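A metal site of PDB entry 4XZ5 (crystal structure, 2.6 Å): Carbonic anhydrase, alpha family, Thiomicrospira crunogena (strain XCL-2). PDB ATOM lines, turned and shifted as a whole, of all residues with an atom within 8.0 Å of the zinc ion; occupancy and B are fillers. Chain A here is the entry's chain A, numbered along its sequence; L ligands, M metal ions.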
ATOM      1  N   TYR A   6     -25.508  38.105 -29.308  1.00  0.00           N
ATOM      2  CA  TYR A   6     -24.535  38.501 -28.299  1.00  0.00           C
ATOM      3  C   TYR A   6     -24.147  39.977 -28.342  1.00  0.00           C
ATOM      4  O   TYR A   6     -23.255  40.401 -27.607  1.00  0.00           O
ATOM      5  CB  TYR A   6     -23.288  37.633 -28.415  1.00  0.00           C
ATOM      6  CG  TYR A   6     -23.544  36.217 -27.948  1.00  0.00           C
ATOM      7  CD1 TYR A   6     -23.432  35.894 -26.604  1.00  0.00           C
ATOM      8  CD2 TYR A   6     -23.923  35.216 -28.838  1.00  0.00           C
ATOM      9  CE1 TYR A   6     -23.667  34.613 -26.162  1.00  0.00           C
ATOM     10  CE2 TYR A   6     -24.159  33.918 -28.393  1.00  0.00           C
ATOM     11  CZ  TYR A   6     -24.025  33.624 -27.047  1.00  0.00           C
ATOM     12  OH  TYR A   6     -24.250  32.348 -26.579  1.00  0.00           O
ATOM     13  N   THR A  67     -23.378  29.002 -32.412  1.00  0.00           N
ATOM     14  CA  THR A  67     -22.195  28.211 -32.089  1.00  0.00           C
ATOM     15  C   THR A  67     -21.887  27.169 -33.183  1.00  0.00           C
ATOM     16  O   THR A  67     -22.654  26.960 -34.117  1.00  0.00           O
ATOM     17  CB  THR A  67     -22.371  27.475 -30.724  1.00  0.00           C
ATOM     18  OG1 THR A  67     -21.155  26.837 -30.310  1.00  0.00           O
ATOM     19  CG2 THR A  67     -23.475  26.436 -30.813  1.00  0.00           C
ATOM     20  N   GLN A  89     -24.907  16.425 -27.661  1.00  0.00           N
ATOM     21  CA  GLN A  89     -24.099  17.297 -28.489  1.00  0.00           C
ATOM     22  C   GLN A  89     -22.984  17.979 -27.736  1.00  0.00           C
ATOM     23  O   GLN A  89     -22.969  18.007 -26.515  1.00  0.00           O
ATOM     24  CB  GLN A  89     -24.971  18.353 -29.157  1.00  0.00           C
ATOM     25  CG  GLN A  89     -25.863  19.168 -28.247  1.00  0.00           C
ATOM     26  CD  GLN A  89     -25.289  20.506 -27.870  1.00  0.00           C
ATOM     27  OE1 GLN A  89     -24.106  20.774 -28.062  1.00  0.00           O
ATOM     28  NE2 GLN A  89     -26.133  21.389 -27.380  1.00  0.00           N
ATOM     29  N   TYR A  90     -22.016  18.489 -28.480  1.00  0.00           N
ATOM     30  CA  TYR A  90     -21.115  19.456 -27.883  1.00  0.00           C
ATOM     31  C   TYR A  90     -20.883  20.631 -28.800  1.00  0.00           C
ATOM     32  O   TYR A  90     -21.051  20.547 -30.010  1.00  0.00           O
ATOM     33  CB  TYR A  90     -19.799  18.811 -27.479  1.00  0.00           C
ATOM     34  CG  TYR A  90     -18.950  18.194 -28.561  1.00  0.00           C
ATOM     35  CD1 TYR A  90     -18.085  18.980 -29.304  1.00  0.00           C
ATOM     36  CD2 TYR A  90     -18.941  16.821 -28.768  1.00  0.00           C
ATOM     37  CE1 TYR A  90     -17.260  18.424 -30.263  1.00  0.00           C
ATOM     38  CE2 TYR A  90     -18.118  16.255 -29.717  1.00  0.00           C
ATOM     39  CZ  TYR A  90     -17.280  17.059 -30.468  1.00  0.00           C
ATOM     40  OH  TYR A  90     -16.454  16.512 -31.437  1.00  0.00           O
ATOM     41  N   HIS A  91     -20.524  21.752 -28.203  1.00  0.00           N
ATOM     42  CA  HIS A  91     -20.402  22.984 -28.946  1.00  0.00           C
ATOM     43  C   HIS A  91     -19.367  23.868 -28.258  1.00  0.00           C
ATOM     44  O   HIS A  91     -18.880  23.523 -27.180  1.00  0.00           O
ATOM     45  CB  HIS A  91     -21.761  23.670 -29.061  1.00  0.00           C
ATOM     46  CG  HIS A  91     -22.347  24.074 -27.747  1.00  0.00           C
ATOM     47  ND1 HIS A  91     -23.149  23.250 -26.999  1.00  0.00           N
ATOM     48  CD2 HIS A  91     -22.226  25.222 -27.034  1.00  0.00           C
ATOM     49  CE1 HIS A  91     -23.496  23.869 -25.883  1.00  0.00           C
ATOM     50  NE2 HIS A  91     -22.954  25.064 -25.885  1.00  0.00           N
ATOM     51  N   PHE A  92     -19.036  25.009 -28.877  1.00  0.00           N
ATOM     52  CA  PHE A  92     -17.887  25.810 -28.438  1.00  0.00           C
ATOM     53  C   PHE A  92     -18.199  27.275 -28.192  1.00  0.00           C
ATOM     54  O   PHE A  92     -19.042  27.857 -28.865  1.00  0.00           O
ATOM     55  CB  PHE A  92     -16.763  25.725 -29.480  1.00  0.00           C
ATOM     56  CG  PHE A  92     -16.241  24.346 -29.688  1.00  0.00           C
ATOM     57  CD1 PHE A  92     -16.854  23.480 -30.575  1.00  0.00           C
ATOM     58  CD2 PHE A  92     -15.122  23.905 -28.983  1.00  0.00           C
ATOM     59  CE1 PHE A  92     -16.346  22.182 -30.768  1.00  0.00           C
ATOM     60  CE2 PHE A  92     -14.615  22.614 -29.169  1.00  0.00           C
ATOM     61  CZ  PHE A  92     -15.235  21.760 -30.056  1.00  0.00           C
ATOM     62  N   HIS A  93     -17.487  27.867 -27.235  1.00  0.00           N
ATOM     63  CA  HIS A  93     -17.582  29.292 -26.962  1.00  0.00           C
ATOM     64  C   HIS A  93     -16.215  29.935 -27.003  1.00  0.00           C
ATOM     65  O   HIS A  93     -15.265  29.412 -26.423  1.00  0.00           O
ATOM     66  CB  HIS A  93     -18.220  29.541 -25.607  1.00  0.00           C
ATOM     67  CG  HIS A  93     -19.581  28.961 -25.456  1.00  0.00           C
ATOM     68  ND1 HIS A  93     -20.734  29.683 -25.701  1.00  0.00           N
ATOM     69  CD2 HIS A  93     -19.986  27.724 -25.068  1.00  0.00           C
ATOM     70  CE1 HIS A  93     -21.787  28.908 -25.479  1.00  0.00           C
ATOM     71  NE2 HIS A  93     -21.369  27.729 -25.091  1.00  0.00           N
ATOM     72  N   GLU A  97     -16.934  30.977 -21.201  1.00  0.00           N
ATOM     73  CA  GLU A  97     -18.046  31.577 -20.472  1.00  0.00           C
ATOM     74  C   GLU A  97     -17.759  31.615 -18.962  1.00  0.00           C
ATOM     75  O   GLU A  97     -17.965  32.628 -18.323  1.00  0.00           O
ATOM     76  CB  GLU A  97     -19.334  30.837 -20.788  1.00  0.00           C
ATOM     77  CG  GLU A  97     -19.808  31.103 -22.206  1.00  0.00           C
ATOM     78  CD  GLU A  97     -21.218  30.592 -22.489  1.00  0.00           C
ATOM     79  OE1 GLU A  97     -21.475  29.399 -22.232  1.00  0.00           O
ATOM     80  OE2 GLU A  97     -22.067  31.388 -22.949  1.00  0.00           O
ATOM     81  N   GLU A 108     -14.098  27.788 -24.566  1.00  0.00           N
ATOM     82  CA  GLU A 108     -14.750  26.837 -23.679  1.00  0.00           C
ATOM     83  C   GLU A 108     -15.596  25.883 -24.502  1.00  0.00           C
ATOM     84  O   GLU A 108     -16.105  26.223 -25.578  1.00  0.00           O
ATOM     85  CB  GLU A 108     -15.615  27.561 -22.625  1.00  0.00           C
ATOM     86  CG  GLU A 108     -16.234  26.630 -21.578  1.00  0.00           C
ATOM     87  CD  GLU A 108     -16.834  27.383 -20.374  1.00  0.00           C
ATOM     88  OE1 GLU A 108     -16.396  28.525 -20.069  1.00  0.00           O
ATOM     89  OE2 GLU A 108     -17.744  26.814 -19.736  1.00  0.00           O
ATOM     90  N   MET A 109     -15.756  24.673 -23.980  1.00  0.00           N
ATOM     91  CA  MET A 109     -16.456  23.617 -24.689  1.00  0.00           C
ATOM     92  C   MET A 109     -17.533  22.969 -23.799  1.00  0.00           C
ATOM     93  O   MET A 109     -17.280  22.664 -22.632  1.00  0.00           O
ATOM     94  CB  MET A 109     -15.425  22.595 -25.154  1.00  0.00           C
ATOM     95  CG  MET A 109     -15.981  21.463 -25.971  1.00  0.00           C
ATOM     96  SD  MET A 109     -14.685  20.255 -26.216  1.00  0.00           S
ATOM     97  CE  MET A 109     -15.678  18.843 -26.672  1.00  0.00           C
ATOM     98  N   HIS A 110     -18.731  22.759 -24.331  1.00  0.00           N
ATOM     99  CA  HIS A 110     -19.801  22.218 -23.524  1.00  0.00           C
ATOM    100  C   HIS A 110     -20.297  20.927 -24.090  1.00  0.00           C
ATOM    101  O   HIS A 110     -20.743  20.915 -25.237  1.00  0.00           O
ATOM    102  CB  HIS A 110     -20.961  23.226 -23.399  1.00  0.00           C
ATOM    103  CG  HIS A 110     -20.603  24.450 -22.634  1.00  0.00           C
ATOM    104  ND1 HIS A 110     -21.279  25.645 -22.764  1.00  0.00           N
ATOM    105  CD2 HIS A 110     -19.652  24.666 -21.684  1.00  0.00           C
ATOM    106  CE1 HIS A 110     -20.740  26.547 -21.954  1.00  0.00           C
ATOM    107  NE2 HIS A 110     -19.754  25.974 -21.287  1.00  0.00           N
ATOM    108  N   LEU A 111     -20.216  19.849 -23.295  1.00  0.00           N
ATOM    109  CA  LEU A 111     -20.796  18.540 -23.675  1.00  0.00           C
ATOM    110  C   LEU A 111     -22.150  18.366 -22.987  1.00  0.00           C
ATOM    111  O   LEU A 111     -22.225  18.138 -21.770  1.00  0.00           O
ATOM    112  CB  LEU A 111     -19.849  17.389 -23.292  1.00  0.00           C
ATOM    113  CG  LEU A 111     -18.566  17.252 -24.111  1.00  0.00           C
ATOM    114  CD1 LEU A 111     -17.472  18.162 -23.576  1.00  0.00           C
ATOM    115  CD2 LEU A 111     -18.085  15.803 -24.088  1.00  0.00           C
ATOM    116  N   VAL A 112     -23.220  18.416 -23.782  1.00  0.00           N
ATOM    117  CA  VAL A 112     -24.558  18.462 -23.226  1.00  0.00           C
ATOM    118  C   VAL A 112     -25.247  17.095 -23.117  1.00  0.00           C
ATOM    119  O   VAL A 112     -25.364  16.357 -24.107  1.00  0.00           O
ATOM    120  CB  VAL A 112     -25.449  19.403 -24.067  1.00  0.00           C
ATOM    121  CG1 VAL A 112     -26.798  19.624 -23.375  1.00  0.00           C
ATOM    122  CG2 VAL A 112     -24.765  20.731 -24.252  1.00  0.00           C
ATOM    123  N   VAL A 122     -24.206  19.005 -17.766  1.00  0.00           N
ATOM    124  CA  VAL A 122     -23.230  19.524 -18.708  1.00  0.00           C
ATOM    125  C   VAL A 122     -21.815  19.410 -18.184  1.00  0.00           C
ATOM    126  O   VAL A 122     -21.513  19.764 -17.039  1.00  0.00           O
ATOM    127  CB  VAL A 122     -23.537  20.995 -19.085  1.00  0.00           C
ATOM    128  CG1 VAL A 122     -22.560  21.523 -20.185  1.00  0.00           C
ATOM    129  CG2 VAL A 122     -24.954  21.120 -19.550  1.00  0.00           C
ATOM    130  N   ILE A 123     -20.939  18.911 -19.050  1.00  0.00           N
ATOM    131  CA  ILE A 123     -19.522  18.878 -18.773  1.00  0.00           C
ATOM    132  C   ILE A 123     -18.864  20.015 -19.580  1.00  0.00           C
ATOM    133  O   ILE A 123     -18.983  20.066 -20.810  1.00  0.00           O
ATOM    134  CB  ILE A 123     -18.887  17.526 -19.156  1.00  0.00           C
ATOM    135  CG1 ILE A 123     -19.540  16.394 -18.383  1.00  0.00           C
ATOM    136  CG2 ILE A 123     -17.373  17.569 -18.948  1.00  0.00           C
ATOM    137  CD1 ILE A 123     -19.036  15.055 -18.753  1.00  0.00           C
ATOM    138  N   ALA A 124     -18.168  20.890 -18.867  1.00  0.00           N
ATOM    139  CA  ALA A 124     -17.454  22.030 -19.464  1.00  0.00           C
ATOM    140  C   ALA A 124     -15.946  21.795 -19.445  1.00  0.00           C
ATOM    141  O   ALA A 124     -15.393  21.320 -18.440  1.00  0.00           O
ATOM    142  CB  ALA A 124     -17.786  23.299 -18.719  1.00  0.00           C
ATOM    143  N   SER A 176     -27.716  26.760 -15.002  1.00  0.00           N
ATOM    144  CA  SER A 176     -28.657  26.884 -16.080  1.00  0.00           C
ATOM    145  C   SER A 176     -27.960  26.751 -17.434  1.00  0.00           C
ATOM    146  O   SER A 176     -26.735  26.644 -17.514  1.00  0.00           O
ATOM    147  CB  SER A 176     -29.375  28.239 -16.004  1.00  0.00           C
ATOM    148  OG  SER A 176     -28.528  29.285 -16.454  1.00  0.00           O
ATOM    149  N   LEU A 177     -28.763  26.766 -18.494  1.00  0.00           N
ATOM    150  CA  LEU A 177     -28.256  27.004 -19.829  1.00  0.00           C
ATOM    151  C   LEU A 177     -27.658  28.407 -19.899  1.00  0.00           C
ATOM    152  O   LEU A 177     -28.119  29.310 -19.189  1.00  0.00           O
ATOM    153  CB  LEU A 177     -29.389  26.891 -20.839  1.00  0.00           C
ATOM    154  CG  LEU A 177     -30.104  25.556 -20.842  1.00  0.00           C
ATOM    155  CD1 LEU A 177     -31.284  25.650 -21.800  1.00  0.00           C
ATOM    156  CD2 LEU A 177     -29.149  24.419 -21.193  1.00  0.00           C
ATOM    157  N   THR A 178     -26.664  28.604 -20.760  1.00  0.00           N
ATOM    158  CA  THR A 178     -26.051  29.922 -20.899  1.00  0.00           C
ATOM    159  C   THR A 178     -26.603  30.678 -22.116  1.00  0.00           C
ATOM    160  O   THR A 178     -26.136  31.768 -22.457  1.00  0.00           O
ATOM    161  CB  THR A 178     -24.525  29.825 -20.980  1.00  0.00           C
ATOM    162  OG1 THR A 178     -24.162  28.995 -22.088  1.00  0.00           O
ATOM    163  CG2 THR A 178     -23.971  29.245 -19.702  1.00  0.00           C
ATOM    164  N   THR A 179     -27.592  30.072 -22.757  1.00  0.00           N
ATOM    165  CA  THR A 179     -28.311  30.661 -23.876  1.00  0.00           C
ATOM    166  C   THR A 179     -29.788  30.626 -23.559  1.00  0.00           C
ATOM    167  O   THR A 179     -30.217  29.747 -22.823  1.00  0.00           O
ATOM    168  CB  THR A 179     -28.098  29.895 -25.175  1.00  0.00           C
ATOM    169  OG1 THR A 179     -28.635  28.595 -25.016  1.00  0.00           O
ATOM    170  CG2 THR A 179     -26.639  29.797 -25.484  1.00  0.00           C
ATOM    171  N   TRP A 188     -23.957  21.154 -13.566  1.00  0.00           N
ATOM    172  CA  TRP A 188     -22.715  21.566 -14.242  1.00  0.00           C
ATOM    173  C   TRP A 188     -21.511  20.900 -13.610  1.00  0.00           C
ATOM    174  O   TRP A 188     -21.358  20.919 -12.405  1.00  0.00           O
ATOM    175  CB  TRP A 188     -22.527  23.093 -14.189  1.00  0.00           C
ATOM    176  CG  TRP A 188     -23.273  23.853 -15.259  1.00  0.00           C
ATOM    177  CD1 TRP A 188     -24.522  24.394 -15.161  1.00  0.00           C
ATOM    178  CD2 TRP A 188     -22.808  24.164 -16.589  1.00  0.00           C
ATOM    179  NE1 TRP A 188     -24.875  25.018 -16.344  1.00  0.00           N
ATOM    180  CE2 TRP A 188     -23.839  24.890 -17.234  1.00  0.00           C
ATOM    181  CE3 TRP A 188     -21.631  23.902 -17.289  1.00  0.00           C
ATOM    182  CZ2 TRP A 188     -23.724  25.350 -18.548  1.00  0.00           C
ATOM    183  CZ3 TRP A 188     -21.518  24.377 -18.589  1.00  0.00           C
ATOM    184  CH2 TRP A 188     -22.561  25.086 -19.203  1.00  0.00           C
ATOM    185  N   ASN A 212     -19.241  34.649 -28.611  1.00  0.00           N
ATOM    186  CA  ASN A 212     -20.541  34.045 -28.296  1.00  0.00           C
ATOM    187  C   ASN A 212     -20.632  33.558 -26.846  1.00  0.00           C
ATOM    188  O   ASN A 212     -21.210  32.482 -26.579  1.00  0.00           O
ATOM    189  CB  ASN A 212     -20.833  32.886 -29.254  1.00  0.00           C
ATOM    190  CG  ASN A 212     -19.827  31.734 -29.128  1.00  0.00           C
ATOM    191  OD1 ASN A 212     -18.697  31.900 -28.629  1.00  0.00           O
ATOM    192  ND2 ASN A 212     -20.258  30.554 -29.538  1.00  0.00           N
HETATM  193  C1  LIG L   1     -25.257  25.688 -22.737  1.00  0.00           C
HETATM  194  O1  LIG L   1     -26.156  26.315 -22.186  1.00  0.00           O
HETATM  195  O2  LIG L   1     -24.922  24.507 -22.709  1.00  0.00           O
HETATM  196  O3  LIG L   1     -24.441  26.488 -23.633  1.00  0.00           O
HETATM  197 ZN    ZN M   1     -22.579  26.206 -24.222  1.00  0.00          ZN
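Residues that only touch the zinc ion: Thr 178 (3.9 Å) and Glu 97 (3.9 Å).
A ring nitrogen (NE2) of His 110 sits at hydrogen-bond distance from the side-chain carboxylate of Glu 108 (2.7 Å). ND1 of His 91 lies within hydrogen-bond range of OE1 of Gln 89, 2.9 Å away. The side-chain carboxylate of Glu 97 lies close to a ring nitrogen (NE2) of His 93 (3.3 Å). N of His 93 sits at hydrogen-bond distance from O of Glu 108. The backbone carbonyl oxygen of Asn 212 lies within hydrogen-bond range of a ring nitrogen (ND1) of His 93. OE1 of Glu 97 is in hydrogen-bond range of OG1 of Thr 178 (2.7 Å). The side-chain carboxylate (OE1) of Glu 108 is in hydrogen-bond range of the backbone NH (N) of Glu 97 (2.8 Å).
The zinc ion is bound by an oxygen (O3) of the ligand, a ring nitrogen (ND1) of His 110, a ring nitrogen (NE2) of His 91 and a ring nitrogen (NE2) of His 93.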
